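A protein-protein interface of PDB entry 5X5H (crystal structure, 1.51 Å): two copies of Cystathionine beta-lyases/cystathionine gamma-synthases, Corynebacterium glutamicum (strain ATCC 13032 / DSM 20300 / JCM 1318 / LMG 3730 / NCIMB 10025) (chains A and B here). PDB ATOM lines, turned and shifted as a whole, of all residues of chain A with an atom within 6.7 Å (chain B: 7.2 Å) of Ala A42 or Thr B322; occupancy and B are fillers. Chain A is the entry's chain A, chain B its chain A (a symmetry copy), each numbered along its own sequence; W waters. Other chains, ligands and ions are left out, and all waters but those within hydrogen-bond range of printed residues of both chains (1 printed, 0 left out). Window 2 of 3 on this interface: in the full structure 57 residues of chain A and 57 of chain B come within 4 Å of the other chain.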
ATOM      1  N   GLN A  40      12.212 -14.977  -8.934  1.00  0.00           N
ATOM      2  CA  GLN A  40      10.862 -14.611  -8.478  1.00  0.00           C
ATOM      3  C   GLN A  40      10.860 -13.250  -7.877  1.00  0.00           C
ATOM      4  O   GLN A  40      11.864 -12.809  -7.334  1.00  0.00           O
ATOM      5  CB  GLN A  40      10.429 -15.670  -7.510  1.00  0.00           C
ATOM      6  CG  GLN A  40      10.360 -17.098  -8.132  1.00  0.00           C
ATOM      7  CD  GLN A  40       9.790 -18.256  -7.403  1.00  0.00           C
ATOM      8  OE1 GLN A  40      10.047 -19.490  -7.705  1.00  0.00           O
ATOM      9  NE2 GLN A  40       9.037 -17.959  -6.425  1.00  0.00           N
ATOM     10  N   ASN A  41       9.699 -12.630  -7.849  1.00  0.00           N
ATOM     11  CA  ASN A  41       9.601 -11.280  -7.272  1.00  0.00           C
ATOM     12  C   ASN A  41       9.400 -11.405  -5.739  1.00  0.00           C
ATOM     13  O   ASN A  41       9.815 -10.468  -5.043  1.00  0.00           O
ATOM     14  CB  ASN A  41       8.370 -10.572  -7.866  1.00  0.00           C
ATOM     15  CG  ASN A  41       8.479 -10.316  -9.358  1.00  0.00           C
ATOM     16  OD1 ASN A  41       9.561 -10.239  -9.871  1.00  0.00           O
ATOM     17  ND2 ASN A  41       7.350 -10.048 -10.057  1.00  0.00           N
ATOM     18  N   ALA A  42       8.853 -12.462  -5.214  1.00  0.00           N
ATOM     19  CA  ALA A  42       8.770 -12.799  -3.788  1.00  0.00           C
ATOM     20  C   ALA A  42       8.552 -14.293  -3.689  1.00  0.00           C
ATOM     21  O   ALA A  42       8.320 -14.913  -4.760  1.00  0.00           O
ATOM     22  CB  ALA A  42       7.581 -12.026  -3.200  1.00  0.00           C
ATOM     23  N   PRO A  43       8.606 -14.974  -2.538  1.00  0.00           N
ATOM     24  CA  PRO A  43       8.511 -16.351  -2.509  1.00  0.00           C
ATOM     25  C   PRO A  43       7.226 -16.860  -3.121  1.00  0.00           C
ATOM     26  O   PRO A  43       6.149 -16.483  -2.642  1.00  0.00           O
ATOM     27  CB  PRO A  43       8.668 -16.720  -0.986  1.00  0.00           C
ATOM     28  CG  PRO A  43       9.508 -15.685  -0.475  1.00  0.00           C
ATOM     29  CD  PRO A  43       8.967 -14.436  -1.163  1.00  0.00           C
ATOM     30  N   ASN A  44       7.372 -17.758  -4.087  1.00  0.00           N
ATOM     31  CA  ASN A  44       6.313 -18.318  -4.928  1.00  0.00           C
ATOM     32  C   ASN A  44       5.410 -17.259  -5.593  1.00  0.00           C
ATOM     33  O   ASN A  44       4.220 -17.501  -5.835  1.00  0.00           O
ATOM     34  CB  ASN A  44       5.515 -19.345  -4.104  1.00  0.00           C
ATOM     35  CG  ASN A  44       4.744 -20.322  -4.996  1.00  0.00           C
ATOM     36  OD1 ASN A  44       5.321 -20.994  -5.898  1.00  0.00           O
ATOM     37  ND2 ASN A  44       3.455 -20.508  -4.660  1.00  0.00           N
ATOM     38  N   GLU A  45       5.916 -16.088  -5.914  1.00  0.00           N
ATOM     39  CA  GLU A  45       5.323 -15.047  -6.763  1.00  0.00           C
ATOM     40  C   GLU A  45       6.219 -14.886  -8.033  1.00  0.00           C
ATOM     41  O   GLU A  45       7.204 -14.173  -8.059  1.00  0.00           O
ATOM     42  CB  GLU A  45       5.229 -13.714  -6.061  1.00  0.00           C
ATOM     43  CG  GLU A  45       4.362 -13.900  -4.835  1.00  0.00           C
ATOM     44  CD  GLU A  45       3.988 -12.651  -4.093  1.00  0.00           C
ATOM     45  OE1 GLU A  45       4.086 -11.536  -4.656  1.00  0.00           O
ATOM     46  OE2 GLU A  45       3.657 -12.842  -2.888  1.00  0.00           O
ATOM     47  N   LEU A  46       5.739 -15.541  -9.095  1.00  0.00           N
ATOM     48  CA  LEU A  46       6.537 -15.671 -10.294  1.00  0.00           C
ATOM     49  C   LEU A  46       6.559 -14.407 -11.062  1.00  0.00           C
ATOM     50  O   LEU A  46       5.611 -13.605 -11.139  1.00  0.00           O
ATOM     51  CB  LEU A  46       6.059 -16.873 -11.080  1.00  0.00           C
ATOM     52  CG  LEU A  46       5.899 -18.218 -10.379  1.00  0.00           C
ATOM     53  CD1 LEU A  46       5.571 -19.366 -11.356  1.00  0.00           C
ATOM     54  CD2 LEU A  46       7.018 -18.624  -9.472  1.00  0.00           C
ATOM     55  N   ALA B 316      10.166 -13.154   8.964  1.00  0.00           N
ATOM     56  CA  ALA B 316      11.599 -12.845   8.849  1.00  0.00           C
ATOM     57  C   ALA B 316      12.249 -13.636   7.734  1.00  0.00           C
ATOM     58  O   ALA B 316      13.013 -12.984   6.968  1.00  0.00           O
ATOM     59  CB  ALA B 316      12.345 -13.157  10.134  1.00  0.00           C
ATOM     60  N   ALA B 317      11.901 -14.915   7.637  1.00  0.00           N
ATOM     61  CA  ALA B 317      12.440 -15.812   6.534  1.00  0.00           C
ATOM     62  C   ALA B 317      12.092 -15.205   5.162  1.00  0.00           C
ATOM     63  O   ALA B 317      12.966 -15.042   4.305  1.00  0.00           O
ATOM     64  CB  ALA B 317      11.944 -17.151   6.665  1.00  0.00           C
ATOM     65  N   LYS B 318      10.842 -14.775   4.951  1.00  0.00           N
ATOM     66  CA  LYS B 318      10.437 -14.212   3.703  1.00  0.00           C
ATOM     67  C   LYS B 318      11.000 -12.889   3.416  1.00  0.00           C
ATOM     68  O   LYS B 318      11.366 -12.575   2.277  1.00  0.00           O
ATOM     69  CB  LYS B 318       8.904 -14.210   3.552  1.00  0.00           C
ATOM     70  CG  LYS B 318       8.329 -15.556   3.521  1.00  0.00           C
ATOM     71  CD  LYS B 318       6.794 -15.417   3.389  1.00  0.00           C
ATOM     72  CE  LYS B 318       6.465 -15.393   1.917  1.00  0.00           C
ATOM     73  NZ  LYS B 318       4.950 -15.379   1.716  1.00  0.00           N
ATOM     74  N   LYS B 319      11.141 -12.027   4.440  1.00  0.00           N
ATOM     75  CA  LYS B 319      11.755 -10.721   4.237  1.00  0.00           C
ATOM     76  C   LYS B 319      13.283 -10.871   3.843  1.00  0.00           C
ATOM     77  O   LYS B 319      13.810 -10.072   3.018  1.00  0.00           O
ATOM     78  CB  LYS B 319      11.604  -9.862   5.522  1.00  0.00           C
ATOM     79  CG  LYS B 319      12.179  -8.468   5.434  1.00  0.00           C
ATOM     80  CD  LYS B 319      11.587  -7.691   4.272  1.00  0.00           C
ATOM     81  CE  LYS B 319      11.983  -6.205   4.186  1.00  0.00           C
ATOM     82  NZ  LYS B 319      12.238  -5.443   5.472  1.00  0.00           N
ATOM     83  N   PHE B 320      13.916 -11.875   4.495  1.00  0.00           N
ATOM     84  CA  PHE B 320      15.350 -12.155   4.152  1.00  0.00           C
ATOM     85  C   PHE B 320      15.411 -12.537   2.648  1.00  0.00           C
ATOM     86  O   PHE B 320      16.274 -12.016   1.937  1.00  0.00           O
ATOM     87  CB  PHE B 320      15.905 -13.197   4.993  1.00  0.00           C
ATOM     88  CG  PHE B 320      17.364 -13.472   4.717  1.00  0.00           C
ATOM     89  CD1 PHE B 320      18.363 -12.624   5.182  1.00  0.00           C
ATOM     90  CD2 PHE B 320      17.682 -14.581   3.975  1.00  0.00           C
ATOM     91  CE1 PHE B 320      19.740 -12.961   4.973  1.00  0.00           C
ATOM     92  CE2 PHE B 320      19.033 -14.890   3.730  1.00  0.00           C
ATOM     93  CZ  PHE B 320      20.055 -14.063   4.191  1.00  0.00           C
ATOM     94  N   CYS B 321      14.466 -13.363   2.247  1.00  0.00           N
ATOM     95  CA  CYS B 321      14.390 -13.767   0.842  1.00  0.00           C
ATOM     96  C   CYS B 321      14.282 -12.615  -0.132  1.00  0.00           C
ATOM     97  O   CYS B 321      14.866 -12.700  -1.261  1.00  0.00           O
ATOM     98  CB  CYS B 321      13.306 -14.828   0.621  1.00  0.00           C
ATOM     99  SG  CYS B 321      13.636 -16.412   1.222  1.00  0.00           S
ATOM    100  N   THR B 322      13.559 -11.553   0.186  1.00  0.00           N
ATOM    101  CA  THR B 322      13.392 -10.443  -0.714  1.00  0.00           C
ATOM    102  C   THR B 322      14.362  -9.268  -0.493  1.00  0.00           C
ATOM    103  O   THR B 322      14.343  -8.251  -1.215  1.00  0.00           O
ATOM    104  CB  THR B 322      11.948  -9.866  -0.693  1.00  0.00           C
ATOM    105  OG1 THR B 322      11.707  -9.403   0.648  1.00  0.00           O
ATOM    106  CG2 THR B 322      10.948 -10.962  -1.003  1.00  0.00           C
ATOM    107  N   SER B 323      15.305  -9.413   0.450  1.00  0.00           N
ATOM    108  CA  SER B 323      16.243  -8.360   0.804  1.00  0.00           C
ATOM    109  C   SER B 323      17.646  -8.494   0.183  1.00  0.00           C
ATOM    110  O   SER B 323      18.418  -7.561   0.153  1.00  0.00           O
ATOM    111  CB  SER B 323      16.424  -8.275   2.277  1.00  0.00           C
ATOM    112  OG  SER B 323      15.186  -7.870   2.852  1.00  0.00           O
ATOM    113  N   THR B 324      17.989  -9.725  -0.202  1.00  0.00           N
ATOM    114  CA  THR B 324      19.309  -9.949  -0.795  1.00  0.00           C
ATOM    115  C   THR B 324      19.371  -9.303  -2.160  1.00  0.00           C
ATOM    116  O   THR B 324      18.339  -9.306  -2.934  1.00  0.00           O
ATOM    117  CB  THR B 324      19.667 -11.439  -0.889  1.00  0.00           C
ATOM    118  OG1 THR B 324      18.596 -12.140  -1.555  1.00  0.00           O
ATOM    119  CG2 THR B 324      19.890 -11.990   0.466  1.00  0.00           C
ATOM    120  N   LYS B 325      20.520  -8.759  -2.558  1.00  0.00           N
ATOM    121  CA  LYS B 325      20.688  -8.126  -3.826  1.00  0.00           C
ATOM    122  C   LYS B 325      21.699  -8.798  -4.738  1.00  0.00           C
ATOM    123  O   LYS B 325      21.814  -8.368  -5.884  1.00  0.00           O
ATOM    124  CB  LYS B 325      21.142  -6.707  -3.599  1.00  0.00           C
ATOM    125  CG  LYS B 325      20.109  -5.865  -2.857  1.00  0.00           C
ATOM    126  CD  LYS B 325      20.548  -4.427  -2.750  1.00  0.00           C
ATOM    127  CE  LYS B 325      20.819  -3.739  -4.098  1.00  0.00           C
ATOM    128  NZ  LYS B 325      19.634  -3.691  -5.030  1.00  0.00           N
ATOM    129  N   LEU B 329      16.673 -14.801  -5.452  1.00  0.00           N
ATOM    130  CA  LEU B 329      15.444 -15.581  -5.109  1.00  0.00           C
ATOM    131  C   LEU B 329      14.964 -16.394  -6.306  1.00  0.00           C
ATOM    132  O   LEU B 329      14.417 -15.836  -7.253  1.00  0.00           O
ATOM    133  CB  LEU B 329      14.370 -14.638  -4.612  1.00  0.00           C
ATOM    134  CG  LEU B 329      13.187 -15.431  -4.094  1.00  0.00           C
ATOM    135  CD1 LEU B 329      13.351 -16.324  -2.919  1.00  0.00           C
ATOM    136  CD2 LEU B 329      12.070 -14.408  -3.710  1.00  0.00           C
ATOM    137  N   LEU B 340      18.776 -18.326  -3.338  1.00  0.00           N
ATOM    138  CA  LEU B 340      18.091 -18.703  -2.090  1.00  0.00           C
ATOM    139  C   LEU B 340      16.572 -18.911  -2.333  1.00  0.00           C
ATOM    140  O   LEU B 340      16.058 -18.419  -3.313  1.00  0.00           O
ATOM    141  CB  LEU B 340      18.341 -17.751  -0.900  1.00  0.00           C
ATOM    142  CG  LEU B 340      17.598 -16.429  -0.920  1.00  0.00           C
ATOM    143  CD1 LEU B 340      18.051 -15.622   0.322  1.00  0.00           C
ATOM    144  CD2 LEU B 340      17.708 -15.513  -2.039  1.00  0.00           C
ATOM    145  N   THR B 345       7.154 -22.872   0.774  1.00  0.00           N
ATOM    146  CA  THR B 345       6.232 -22.323  -0.249  1.00  0.00           C
ATOM    147  C   THR B 345       6.755 -22.626  -1.644  1.00  0.00           C
ATOM    148  O   THR B 345       6.050 -22.382  -2.639  1.00  0.00           O
ATOM    149  CB  THR B 345       5.989 -20.791  -0.005  1.00  0.00           C
ATOM    150  OG1 THR B 345       7.240 -20.113  -0.067  1.00  0.00           O
ATOM    151  CG2 THR B 345       5.308 -20.532   1.370  1.00  0.00           C
ATOM    152  N   MET B 346       7.944 -23.168  -1.853  1.00  0.00           N
ATOM    153  CA  MET B 346       8.509 -23.228  -3.129  1.00  0.00           C
ATOM    154  C   MET B 346       8.860 -24.659  -3.351  1.00  0.00           C
ATOM    155  O   MET B 346       7.973 -25.410  -3.660  1.00  0.00           O
ATOM    156  CB  MET B 346       9.791 -22.252  -3.187  1.00  0.00           C
ATOM    157  CG  MET B 346       9.450 -20.756  -3.123  1.00  0.00           C
ATOM    158  SD  MET B 346      10.773 -19.478  -2.965  1.00  0.00           S
ATOM    159  CE  MET B 346      11.662 -19.694  -4.557  1.00  0.00           C
ATOM    160  N   ALA B 382      21.164  -7.802   4.286  1.00  0.00           N
ATOM    161  CA  ALA B 382      19.842  -8.371   4.289  1.00  0.00           C
ATOM    162  C   ALA B 382      19.379  -8.644   5.703  1.00  0.00           C
ATOM    163  O   ALA B 382      18.199  -8.358   6.047  1.00  0.00           O
ATOM    164  CB  ALA B 382      19.811  -9.666   3.484  1.00  0.00           C
ATOM    165  N   ASN B 385      18.200  -5.472   7.272  1.00  0.00           N
ATOM    166  CA  ASN B 385      16.874  -5.089   6.711  1.00  0.00           C
ATOM    167  C   ASN B 385      15.712  -5.728   7.447  1.00  0.00           C
ATOM    168  O   ASN B 385      14.522  -5.442   7.136  1.00  0.00           O
ATOM    169  CB  ASN B 385      16.720  -5.346   5.202  1.00  0.00           C
ATOM    170  CG  ASN B 385      15.746  -4.369   4.499  1.00  0.00           C
ATOM    171  OD1 ASN B 385      15.650  -3.202   4.861  1.00  0.00           O
ATOM    172  ND2 ASN B 385      15.044  -4.853   3.478  1.00  0.00           N
HETATM  173  O   HOH W   1       5.286 -14.597  -0.916  1.00  0.00           O
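The backbone NH (N) of Gln A40 sits at hydrogen-bond distance from the backbone carbonyl oxygen (O) of Leu B329, at 2.9 Å.
The backbone carbonyl oxygen (O) of Lys B319 sits at hydrogen-bond distance from the side-chain hydroxyl (OG1) of Thr B322 (3.2 Å).
The side-chain amide nitrogen (NE2) of Gln A40 lies close to the backbone NH (N) of Asn A44 (2.9 Å).
Among the printed residues, pairs that only touch across the chains: Gln A40 with Met B346 (3.5 Å), Ala A42 with Thr B322 (3.98 Å), Ala A42 with Leu B329 (3.5 Å), Pro A43 with Lys B318 (3.9 Å), Pro A43 with Leu B329 (3.7 Å), Pro A43 with Thr B345 (3.8 Å), Pro A43 with Met B346 (3.9 Å), Asn A44 with Thr B345 (3.4 Å) and Asn A44 with Met B346 (3.8 Å).
Of the printed residues of chain B, Gln A40 touches Leu B329 (2.9 Å) and Met B346 (3.5 Å).
Of the printed residues of chain B, Asn A44 touches Thr B345 (3.4 Å) and Met B346 (3.8 Å).
Of the printed residues of chain A, Lys B318 touches Pro A43.
Printed residues of chain A within 4 Å of Thr B322: Ala A42.
Thr B324 touches none of the printed residues of chain A.
Of the printed residues of chain A, Leu B329 touches Gln A40, Ala A42 and Pro A43.
Asn B385 touches none of the printed residues of chain A.
The nearest printed residue of chain B that does not touch Ala A42 is Met B346 (5.5 Å).
Of the 16 printed residues of chain B, 5 touch a printed residue of chain A.
Hydrophobic or aromatic side chains of chain B within 4 Å of the printed part of chain A: Leu B329 and Met B346.
Of the 7 printed residues of chain A, 4 touch a printed residue of chain B.
Among the printed residues, no Asp or Glu carboxylate lies within 4 Å of a Lys or Arg side-chain nitrogen of the other chain.
No position is printed for both chains.
Water W1 lies within hydrogen-bond range of O of Pro A43 (2.7 Å), NZ of Lys B318 (2.8 Å) and OE2 of Glu A45 (3.1 Å).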
